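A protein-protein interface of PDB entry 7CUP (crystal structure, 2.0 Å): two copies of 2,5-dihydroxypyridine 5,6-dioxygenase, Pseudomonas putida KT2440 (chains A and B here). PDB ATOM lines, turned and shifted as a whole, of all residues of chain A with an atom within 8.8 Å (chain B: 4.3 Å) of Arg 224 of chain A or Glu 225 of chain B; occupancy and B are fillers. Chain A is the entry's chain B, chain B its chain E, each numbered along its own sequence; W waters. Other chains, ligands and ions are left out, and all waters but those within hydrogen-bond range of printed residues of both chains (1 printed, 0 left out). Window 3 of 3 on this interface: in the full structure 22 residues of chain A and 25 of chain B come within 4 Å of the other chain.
The guanidinium group of Arg 224 of chain A is in salt-bridge range of the side-chain carboxylate of Glu 225 of chain B (2.9 Å).
NH1 of Arg 224 of chain A lies within salt-bridge range of OE1 of Glu 244 of chain B.
N of Gly 213 of chain A is in hydrogen-bond range of O of Cys 223 of chain A (2.8 Å).
N of Arg 224 of chain B sits at hydrogen-bond distance from OE1 of Glu 244 of chain B (2.8 Å).
The side-chain carboxylate of Glu 244 of chain A lies within hydrogen-bond range of the backbone NH of Arg 224 of chain A (2.8 Å).
The side-chain carboxylate (OE2) of Glu 244 of chain B lies within hydrogen-bond range of the backbone NH (N) of Glu 225 of chain B, 3.3 Å away.
The backbone NH (N) of Phe 243 of chain B sits at hydrogen-bond distance from the side-chain carboxylate (OE2) of Glu 225 of chain B, 2.9 Å away.
Among the printed residues, pairs that only touch across the chains: Val 212 of chain A with Phe 243 of chain B (3.5 Å), Gly 213 of chain A with Phe 243 of chain B (3.4 Å), Tyr 222 of chain A with Phe 243 of chain B (3.6 Å), Arg 224 of chain A with Arg 224 of chain B (3.97 Å) and Arg 224 of chain A with Phe 243 of chain B (3.5 Å).
Asn 221 of chain A touches none of the printed residues of chain B.
Of the printed residues of chain B, Tyr 222 of chain A touches Phe 243.
Arg 224 of chain A touches just these residues of chain B: Arg 224, Glu 225, Phe 243 and Glu 244.
Of the printed residues of chain A, Arg 224 of chain B touches Arg 224 (3.97 Å).
Of chain A, only Arg 224 (2.9 Å) comes within 4 Å of Glu 225 of chain B.
Printed residues of chain A within 4 Å of Phe 243 of chain B: Val 212 (3.5 Å), Gly 213 (3.4 Å), Tyr 222 (3.6 Å) and Arg 224 (3.5 Å).
The nearest printed residue of chain B that does not touch Arg 224 of chain A is Gly 242 of chain B (6.0 Å).
Of the 18 printed residues of chain A, 4 touch a printed residue of chain B.
Among the printed residues, 7 pairs touch across the chains.
Arg 224 of chain B touches its own counterpart, Arg 224 of chain A.
Arg 224 of chain A touches Glu 225 of chain B, but with the chains exchanged Glu 225 of chain A does not touch Arg 224 of chain B (9.9 Å).
Arg 224 of chain A touches Phe 243 of chain B, but with the chains exchanged Phe 243 of chain A does not touch Arg 224 of chain B (9.6 Å).
Arg 224 of chain A touches Glu 244 of chain B, but with the chains exchanged Glu 244 of chain A does not touch Arg 224 of chain B (9.7 Å).
9 positions are printed for both chains.
Of the 7 pairs that touch across the chains among the printed residues, 1 has its exchanged pair printed and touching as well.
Water W1 lies within hydrogen-bond range of the backbone carbonyl oxygen (O) of Arg 224 of chain A (2.7 Å) and the side-chain carboxylate (OE2) of Glu 225 of chain B (3.4 Å).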
ATOM      1  N   LEU A 210     -19.042  11.386 -16.340  1.00  0.00           N
ATOM      2  CA  LEU A 210     -19.553  10.532 -15.246  1.00  0.00           C
ATOM      3  C   LEU A 210     -19.063  11.181 -13.961  1.00  0.00           C
ATOM      4  O   LEU A 210     -17.866  11.166 -13.714  1.00  0.00           O
ATOM      5  CB  LEU A 210     -19.051   9.092 -15.387  1.00  0.00           C
ATOM      6  CG  LEU A 210     -19.779   8.224 -16.407  1.00  0.00           C
ATOM      7  CD1 LEU A 210     -19.560   8.722 -17.829  1.00  0.00           C
ATOM      8  CD2 LEU A 210     -19.284   6.816 -16.301  1.00  0.00           C
ATOM      9  N   ASP A 211     -19.972  11.788 -13.221  1.00  0.00           N
ATOM     10  CA  ASP A 211     -19.649  12.450 -11.942  1.00  0.00           C
ATOM     11  C   ASP A 211     -19.506  11.376 -10.858  1.00  0.00           C
ATOM     12  O   ASP A 211     -19.870  10.186 -11.121  1.00  0.00           O
ATOM     13  CB  ASP A 211     -20.723  13.474 -11.601  1.00  0.00           C
ATOM     14  CG  ASP A 211     -20.265  14.485 -10.565  1.00  0.00           C
ATOM     15  OD1 ASP A 211     -19.089  14.431 -10.188  1.00  0.00           O
ATOM     16  OD2 ASP A 211     -21.113  15.282 -10.119  1.00  0.00           O
ATOM     17  N   VAL A 212     -18.962  11.785  -9.707  1.00  0.00           N
ATOM     18  CA  VAL A 212     -19.027  11.015  -8.433  1.00  0.00           C
ATOM     19  C   VAL A 212     -20.493  10.620  -8.251  1.00  0.00           C
ATOM     20  O   VAL A 212     -21.351  11.503  -8.341  1.00  0.00           O
ATOM     21  CB  VAL A 212     -18.479  11.822  -7.234  1.00  0.00           C
ATOM     22  CG1 VAL A 212     -18.778  11.140  -5.903  1.00  0.00           C
ATOM     23  CG2 VAL A 212     -16.979  12.064  -7.363  1.00  0.00           C
ATOM     24  N   GLY A 213     -20.776   9.330  -8.107  1.00  0.00           N
ATOM     25  CA  GLY A 213     -22.164   8.866  -7.928  1.00  0.00           C
ATOM     26  C   GLY A 213     -22.773   8.311  -9.197  1.00  0.00           C
ATOM     27  O   GLY A 213     -23.763   7.580  -9.083  1.00  0.00           O
ATOM     28  N   ASP A 214     -22.259   8.636 -10.381  1.00  0.00           N
ATOM     29  CA  ASP A 214     -22.828   8.092 -11.642  1.00  0.00           C
ATOM     30  C   ASP A 214     -22.391   6.638 -11.789  1.00  0.00           C
ATOM     31  O   ASP A 214     -21.499   6.193 -11.069  1.00  0.00           O
ATOM     32  CB  ASP A 214     -22.553   8.996 -12.852  1.00  0.00           C
ATOM     33  CG  ASP A 214     -23.314  10.321 -12.758  1.00  0.00           C
ATOM     34  OD1 ASP A 214     -24.429  10.327 -12.188  1.00  0.00           O
ATOM     35  OD2 ASP A 214     -22.786  11.326 -13.234  1.00  0.00           O
ATOM     36  N   ILE A 215     -23.069   5.900 -12.664  1.00  0.00           N
ATOM     37  CA  ILE A 215     -23.051   4.406 -12.664  1.00  0.00           C
ATOM     38  C   ILE A 215     -22.621   3.950 -14.052  1.00  0.00           C
ATOM     39  O   ILE A 215     -23.118   4.542 -15.028  1.00  0.00           O
ATOM     40  CB  ILE A 215     -24.442   3.866 -12.286  1.00  0.00           C
ATOM     41  CG1 ILE A 215     -24.821   4.264 -10.858  1.00  0.00           C
ATOM     42  CG2 ILE A 215     -24.511   2.365 -12.513  1.00  0.00           C
ATOM     43  CD1 ILE A 215     -26.281   4.101 -10.519  1.00  0.00           C
ATOM     44  N   ASN A 221     -21.145  -0.208 -10.326  1.00  0.00           N
ATOM     45  CA  ASN A 221     -20.637   0.585  -9.192  1.00  0.00           C
ATOM     46  C   ASN A 221     -20.886   2.061  -9.453  1.00  0.00           C
ATOM     47  O   ASN A 221     -21.152   2.489 -10.614  1.00  0.00           O
ATOM     48  CB  ASN A 221     -19.202   0.234  -8.793  1.00  0.00           C
ATOM     49  CG  ASN A 221     -18.316  -0.121  -9.957  1.00  0.00           C
ATOM     50  OD1 ASN A 221     -18.004   0.734 -10.780  1.00  0.00           O
ATOM     51  ND2 ASN A 221     -17.876  -1.367 -10.004  1.00  0.00           N
ATOM     52  N   TYR A 222     -20.885   2.776  -8.344  1.00  0.00           N
ATOM     53  CA  TYR A 222     -21.020   4.239  -8.272  1.00  0.00           C
ATOM     54  C   TYR A 222     -19.621   4.809  -8.427  1.00  0.00           C
ATOM     55  O   TYR A 222     -18.754   4.417  -7.647  1.00  0.00           O
ATOM     56  CB  TYR A 222     -21.626   4.628  -6.925  1.00  0.00           C
ATOM     57  CG  TYR A 222     -23.024   4.124  -6.677  1.00  0.00           C
ATOM     58  CD1 TYR A 222     -24.118   4.852  -7.089  1.00  0.00           C
ATOM     59  CD2 TYR A 222     -23.256   2.969  -5.949  1.00  0.00           C
ATOM     60  CE1 TYR A 222     -25.412   4.452  -6.802  1.00  0.00           C
ATOM     61  CE2 TYR A 222     -24.539   2.521  -5.705  1.00  0.00           C
ATOM     62  CZ  TYR A 222     -25.626   3.275  -6.112  1.00  0.00           C
ATOM     63  OH  TYR A 222     -26.905   2.856  -5.865  1.00  0.00           O
ATOM     64  N   CYS A 223     -19.394   5.672  -9.412  1.00  0.00           N
ATOM     65  CA  CYS A 223     -18.052   6.262  -9.608  1.00  0.00           C
ATOM     66  C   CYS A 223     -17.670   6.991  -8.330  1.00  0.00           C
ATOM     67  O   CYS A 223     -18.522   7.699  -7.787  1.00  0.00           O
ATOM     68  CB  CYS A 223     -18.010   7.213 -10.791  1.00  0.00           C
ATOM     69  SG  CYS A 223     -18.233   6.331 -12.350  1.00  0.00           S
ATOM     70  N   ARG A 224     -16.424   6.826  -7.885  1.00  0.00           N
ATOM     71  CA  ARG A 224     -15.867   7.551  -6.709  1.00  0.00           C
ATOM     72  C   ARG A 224     -14.969   8.699  -7.192  1.00  0.00           C
ATOM     73  O   ARG A 224     -14.676   9.586  -6.376  1.00  0.00           O
ATOM     74  CB  ARG A 224     -15.153   6.557  -5.773  1.00  0.00           C
ATOM     75  CG  ARG A 224     -16.072   5.532  -5.114  1.00  0.00           C
ATOM     76  CD  ARG A 224     -17.332   6.158  -4.510  1.00  0.00           C
ATOM     77  NE  ARG A 224     -17.023   7.131  -3.461  1.00  0.00           N
ATOM     78  CZ  ARG A 224     -17.040   6.888  -2.151  1.00  0.00           C
ATOM     79  NH1 ARG A 224     -17.391   5.699  -1.685  1.00  0.00           N
ATOM     80  NH2 ARG A 224     -16.743   7.856  -1.303  1.00  0.00           N
ATOM     81  N   GLU A 225     -14.605   8.713  -8.473  1.00  0.00           N
ATOM     82  CA  GLU A 225     -13.952   9.865  -9.148  1.00  0.00           C
ATOM     83  C   GLU A 225     -14.549  10.017 -10.550  1.00  0.00           C
ATOM     84  O   GLU A 225     -15.088   9.041 -11.108  1.00  0.00           O
ATOM     85  CB  GLU A 225     -12.420   9.732  -9.205  1.00  0.00           C
ATOM     86  CG  GLU A 225     -11.880   8.358  -8.844  1.00  0.00           C
ATOM     87  CD  GLU A 225     -10.364   8.203  -8.919  1.00  0.00           C
ATOM     88  OE1 GLU A 225      -9.889   7.022  -9.053  1.00  0.00           O
ATOM     89  OE2 GLU A 225      -9.649   9.266  -8.842  1.00  0.00           O
ATOM     90  N   ARG A 226     -14.423  11.215 -11.105  1.00  0.00           N
ATOM     91  CA  ARG A 226     -14.962  11.566 -12.440  1.00  0.00           C
ATOM     92  C   ARG A 226     -14.332  10.712 -13.544  1.00  0.00           C
ATOM     93  O   ARG A 226     -13.137  10.441 -13.505  1.00  0.00           O
ATOM     94  CB  ARG A 226     -14.789  13.066 -12.687  1.00  0.00           C
ATOM     95  CG  ARG A 226     -15.705  13.882 -11.799  1.00  0.00           C
ATOM     96  CD  ARG A 226     -15.633  15.367 -12.019  1.00  0.00           C
ATOM     97  NE  ARG A 226     -16.682  15.985 -11.223  1.00  0.00           N
ATOM     98  CZ  ARG A 226     -16.895  17.290 -11.156  1.00  0.00           C
ATOM     99  NH1 ARG A 226     -16.130  18.119 -11.847  1.00  0.00           N
ATOM    100  NH2 ARG A 226     -17.871  17.760 -10.395  1.00  0.00           N
ATOM    101  N   ILE A 227     -15.142  10.359 -14.535  1.00  0.00           N
ATOM    102  CA  ILE A 227     -14.672   9.931 -15.873  1.00  0.00           C
ATOM    103  C   ILE A 227     -15.213  10.940 -16.881  1.00  0.00           C
ATOM    104  O   ILE A 227     -16.434  11.213 -16.893  1.00  0.00           O
ATOM    105  CB  ILE A 227     -15.075   8.486 -16.209  1.00  0.00           C
ATOM    106  CG1 ILE A 227     -14.752   7.518 -15.065  1.00  0.00           C
ATOM    107  CG2 ILE A 227     -14.412   8.060 -17.523  1.00  0.00           C
ATOM    108  CD1 ILE A 227     -15.067   6.086 -15.389  1.00  0.00           C
ATOM    109  N   GLY A 241      -9.599   9.978 -16.325  1.00  0.00           N
ATOM    110  CA  GLY A 241      -9.834  10.333 -14.903  1.00  0.00           C
ATOM    111  C   GLY A 241      -9.606   9.210 -13.888  1.00  0.00           C
ATOM    112  O   GLY A 241     -10.606   8.626 -13.390  1.00  0.00           O
ATOM    113  N   GLY A 242      -8.364   8.932 -13.508  1.00  0.00           N
ATOM    114  CA  GLY A 242      -8.043   8.017 -12.384  1.00  0.00           C
ATOM    115  C   GLY A 242      -8.477   6.562 -12.573  1.00  0.00           C
ATOM    116  O   GLY A 242      -8.393   6.030 -13.702  1.00  0.00           O
ATOM    117  N   PHE A 243      -8.922   5.906 -11.495  1.00  0.00           N
ATOM    118  CA  PHE A 243      -8.975   4.421 -11.445  1.00  0.00           C
ATOM    119  C   PHE A 243     -10.145   3.923 -12.300  1.00  0.00           C
ATOM    120  O   PHE A 243      -9.946   3.028 -13.122  1.00  0.00           O
ATOM    121  CB  PHE A 243      -9.078   3.890 -10.012  1.00  0.00           C
ATOM    122  CG  PHE A 243      -9.435   2.432  -9.990  1.00  0.00           C
ATOM    123  CD1 PHE A 243      -8.593   1.505 -10.572  1.00  0.00           C
ATOM    124  CD2 PHE A 243     -10.665   2.007  -9.524  1.00  0.00           C
ATOM    125  CE1 PHE A 243      -8.941   0.168 -10.611  1.00  0.00           C
ATOM    126  CE2 PHE A 243     -11.019   0.666  -9.569  1.00  0.00           C
ATOM    127  CZ  PHE A 243     -10.149  -0.252 -10.105  1.00  0.00           C
ATOM    128  N   GLU A 244     -11.337   4.482 -12.081  1.00  0.00           N
ATOM    129  CA  GLU A 244     -12.541   4.103 -12.850  1.00  0.00           C
ATOM    130  C   GLU A 244     -12.193   4.196 -14.345  1.00  0.00           C
ATOM    131  O   GLU A 244     -12.511   3.289 -15.082  1.00  0.00           O
ATOM    132  CB  GLU A 244     -13.753   4.966 -12.490  1.00  0.00           C
ATOM    133  CG  GLU A 244     -14.547   4.529 -11.258  1.00  0.00           C
ATOM    134  CD  GLU A 244     -14.139   5.264 -10.004  1.00  0.00           C
ATOM    135  OE1 GLU A 244     -14.649   4.945  -8.924  1.00  0.00           O
ATOM    136  OE2 GLU A 244     -13.272   6.133 -10.116  1.00  0.00           O
ATOM    137  N   ALA A 245     -11.539   5.262 -14.794  1.00  0.00           N
ATOM    138  CA  ALA A 245     -11.264   5.460 -16.236  1.00  0.00           C
ATOM    139  C   ALA A 245     -10.268   4.401 -16.729  1.00  0.00           C
ATOM    140  O   ALA A 245     -10.481   3.829 -17.828  1.00  0.00           O
ATOM    141  CB  ALA A 245     -10.780   6.873 -16.476  1.00  0.00           C
ATOM    142  N   VAL B 212     -13.981   7.143   8.167  1.00  0.00           N
ATOM    143  CA  VAL B 212     -13.514   6.201   7.138  1.00  0.00           C
ATOM    144  C   VAL B 212     -13.425   4.852   7.846  1.00  0.00           C
ATOM    145  O   VAL B 212     -12.798   4.799   8.895  1.00  0.00           O
ATOM    146  CB  VAL B 212     -12.174   6.674   6.546  1.00  0.00           C
ATOM    147  CG1 VAL B 212     -11.558   5.576   5.707  1.00  0.00           C
ATOM    148  CG2 VAL B 212     -12.320   7.970   5.745  1.00  0.00           C
ATOM    149  N   CYS B 223     -17.365   3.074   4.984  1.00  0.00           N
ATOM    150  CA  CYS B 223     -17.294   4.490   4.545  1.00  0.00           C
ATOM    151  C   CYS B 223     -15.880   4.763   4.037  1.00  0.00           C
ATOM    152  O   CYS B 223     -14.897   4.383   4.690  1.00  0.00           O
ATOM    153  CB  CYS B 223     -17.698   5.423   5.668  1.00  0.00           C
ATOM    154  SG  CYS B 223     -19.455   5.278   6.073  1.00  0.00           S
ATOM    155  N   ARG B 224     -15.774   5.367   2.871  1.00  0.00           N
ATOM    156  CA  ARG B 224     -14.464   5.784   2.319  1.00  0.00           C
ATOM    157  C   ARG B 224     -14.300   7.288   2.535  1.00  0.00           C
ATOM    158  O   ARG B 224     -13.178   7.740   2.435  1.00  0.00           O
ATOM    159  CB  ARG B 224     -14.374   5.313   0.861  1.00  0.00           C
ATOM    160  CG  ARG B 224     -14.485   3.798   0.707  1.00  0.00           C
ATOM    161  CD  ARG B 224     -13.520   3.101   1.650  1.00  0.00           C
ATOM    162  NE  ARG B 224     -12.132   3.483   1.363  1.00  0.00           N
ATOM    163  CZ  ARG B 224     -11.293   2.800   0.581  1.00  0.00           C
ATOM    164  NH1 ARG B 224     -11.663   1.672  -0.002  1.00  0.00           N
ATOM    165  NH2 ARG B 224     -10.073   3.248   0.394  1.00  0.00           N
ATOM    166  N   GLU B 225     -15.396   8.006   2.767  1.00  0.00           N
ATOM    167  CA  GLU B 225     -15.391   9.423   3.222  1.00  0.00           C
ATOM    168  C   GLU B 225     -16.180   9.498   4.526  1.00  0.00           C
ATOM    169  O   GLU B 225     -17.027   8.647   4.720  1.00  0.00           O
ATOM    170  CB  GLU B 225     -16.013  10.331   2.168  1.00  0.00           C
ATOM    171  CG  GLU B 225     -15.486  10.070   0.785  1.00  0.00           C
ATOM    172  CD  GLU B 225     -15.988  11.054  -0.244  1.00  0.00           C
ATOM    173  OE1 GLU B 225     -15.413  12.167  -0.281  1.00  0.00           O
ATOM    174  OE2 GLU B 225     -16.942  10.716  -0.986  1.00  0.00           O
ATOM    175  N   ARG B 226     -15.888  10.474   5.385  1.00  0.00           N
ATOM    176  CA  ARG B 226     -16.623  10.688   6.645  1.00  0.00           C
ATOM    177  C   ARG B 226     -18.034  11.186   6.349  1.00  0.00           C
ATOM    178  O   ARG B 226     -18.270  11.858   5.338  1.00  0.00           O
ATOM    179  CB  ARG B 226     -15.940  11.699   7.565  1.00  0.00           C
ATOM    180  CG  ARG B 226     -14.560  11.294   8.035  1.00  0.00           C
ATOM    181  CD  ARG B 226     -14.057  12.272   9.089  1.00  0.00           C
ATOM    182  NE  ARG B 226     -12.867  11.670   9.672  1.00  0.00           N
ATOM    183  CZ  ARG B 226     -11.670  11.602   9.080  1.00  0.00           C
ATOM    184  NH1 ARG B 226     -11.468  12.139   7.887  1.00  0.00           N
ATOM    185  NH2 ARG B 226     -10.664  11.002   9.693  1.00  0.00           N
ATOM    186  N   ILE B 227     -18.950  10.821   7.225  1.00  0.00           N
ATOM    187  CA  ILE B 227     -20.304  11.413   7.299  1.00  0.00           C
ATOM    188  C   ILE B 227     -20.412  11.983   8.708  1.00  0.00           C
ATOM    189  O   ILE B 227     -20.095  11.262   9.675  1.00  0.00           O
ATOM    190  CB  ILE B 227     -21.395  10.382   7.006  1.00  0.00           C
ATOM    191  CG1 ILE B 227     -21.180   9.676   5.668  1.00  0.00           C
ATOM    192  CG2 ILE B 227     -22.782  11.016   7.096  1.00  0.00           C
ATOM    193  CD1 ILE B 227     -22.180   8.569   5.433  1.00  0.00           C
ATOM    194  N   GLY B 242     -19.218  13.678   1.870  1.00  0.00           N
ATOM    195  CA  GLY B 242     -19.114  13.563   0.407  1.00  0.00           C
ATOM    196  C   GLY B 242     -20.160  12.619  -0.139  1.00  0.00           C
ATOM    197  O   GLY B 242     -21.367  12.834   0.083  1.00  0.00           O
ATOM    198  N   PHE B 243     -19.711  11.582  -0.830  1.00  0.00           N
ATOM    199  CA  PHE B 243     -20.615  10.778  -1.673  1.00  0.00           C
ATOM    200  C   PHE B 243     -21.472   9.919  -0.749  1.00  0.00           C
ATOM    201  O   PHE B 243     -22.679   9.932  -1.007  1.00  0.00           O
ATOM    202  CB  PHE B 243     -19.864   9.991  -2.752  1.00  0.00           C
ATOM    203  CG  PHE B 243     -20.726   8.918  -3.352  1.00  0.00           C
ATOM    204  CD1 PHE B 243     -21.845   9.263  -4.092  1.00  0.00           C
ATOM    205  CD2 PHE B 243     -20.500   7.586  -3.064  1.00  0.00           C
ATOM    206  CE1 PHE B 243     -22.683   8.274  -4.583  1.00  0.00           C
ATOM    207  CE2 PHE B 243     -21.352   6.601  -3.541  1.00  0.00           C
ATOM    208  CZ  PHE B 243     -22.438   6.949  -4.307  1.00  0.00           C
ATOM    209  N   GLU B 244     -20.916   9.277   0.296  1.00  0.00           N
ATOM    210  CA  GLU B 244     -21.724   8.446   1.239  1.00  0.00           C
ATOM    211  C   GLU B 244     -22.833   9.306   1.869  1.00  0.00           C
ATOM    212  O   GLU B 244     -23.954   8.768   2.072  1.00  0.00           O
ATOM    213  CB  GLU B 244     -20.917   7.747   2.339  1.00  0.00           C
ATOM    214  CG  GLU B 244     -20.114   6.533   1.886  1.00  0.00           C
ATOM    215  CD  GLU B 244     -18.696   6.828   1.449  1.00  0.00           C
ATOM    216  OE1 GLU B 244     -17.946   5.874   1.198  1.00  0.00           O
ATOM    217  OE2 GLU B 244     -18.364   8.020   1.282  1.00  0.00           O
HETATM  218  O   HOH W   1     -15.893   9.714  -4.025  1.00  0.00           O
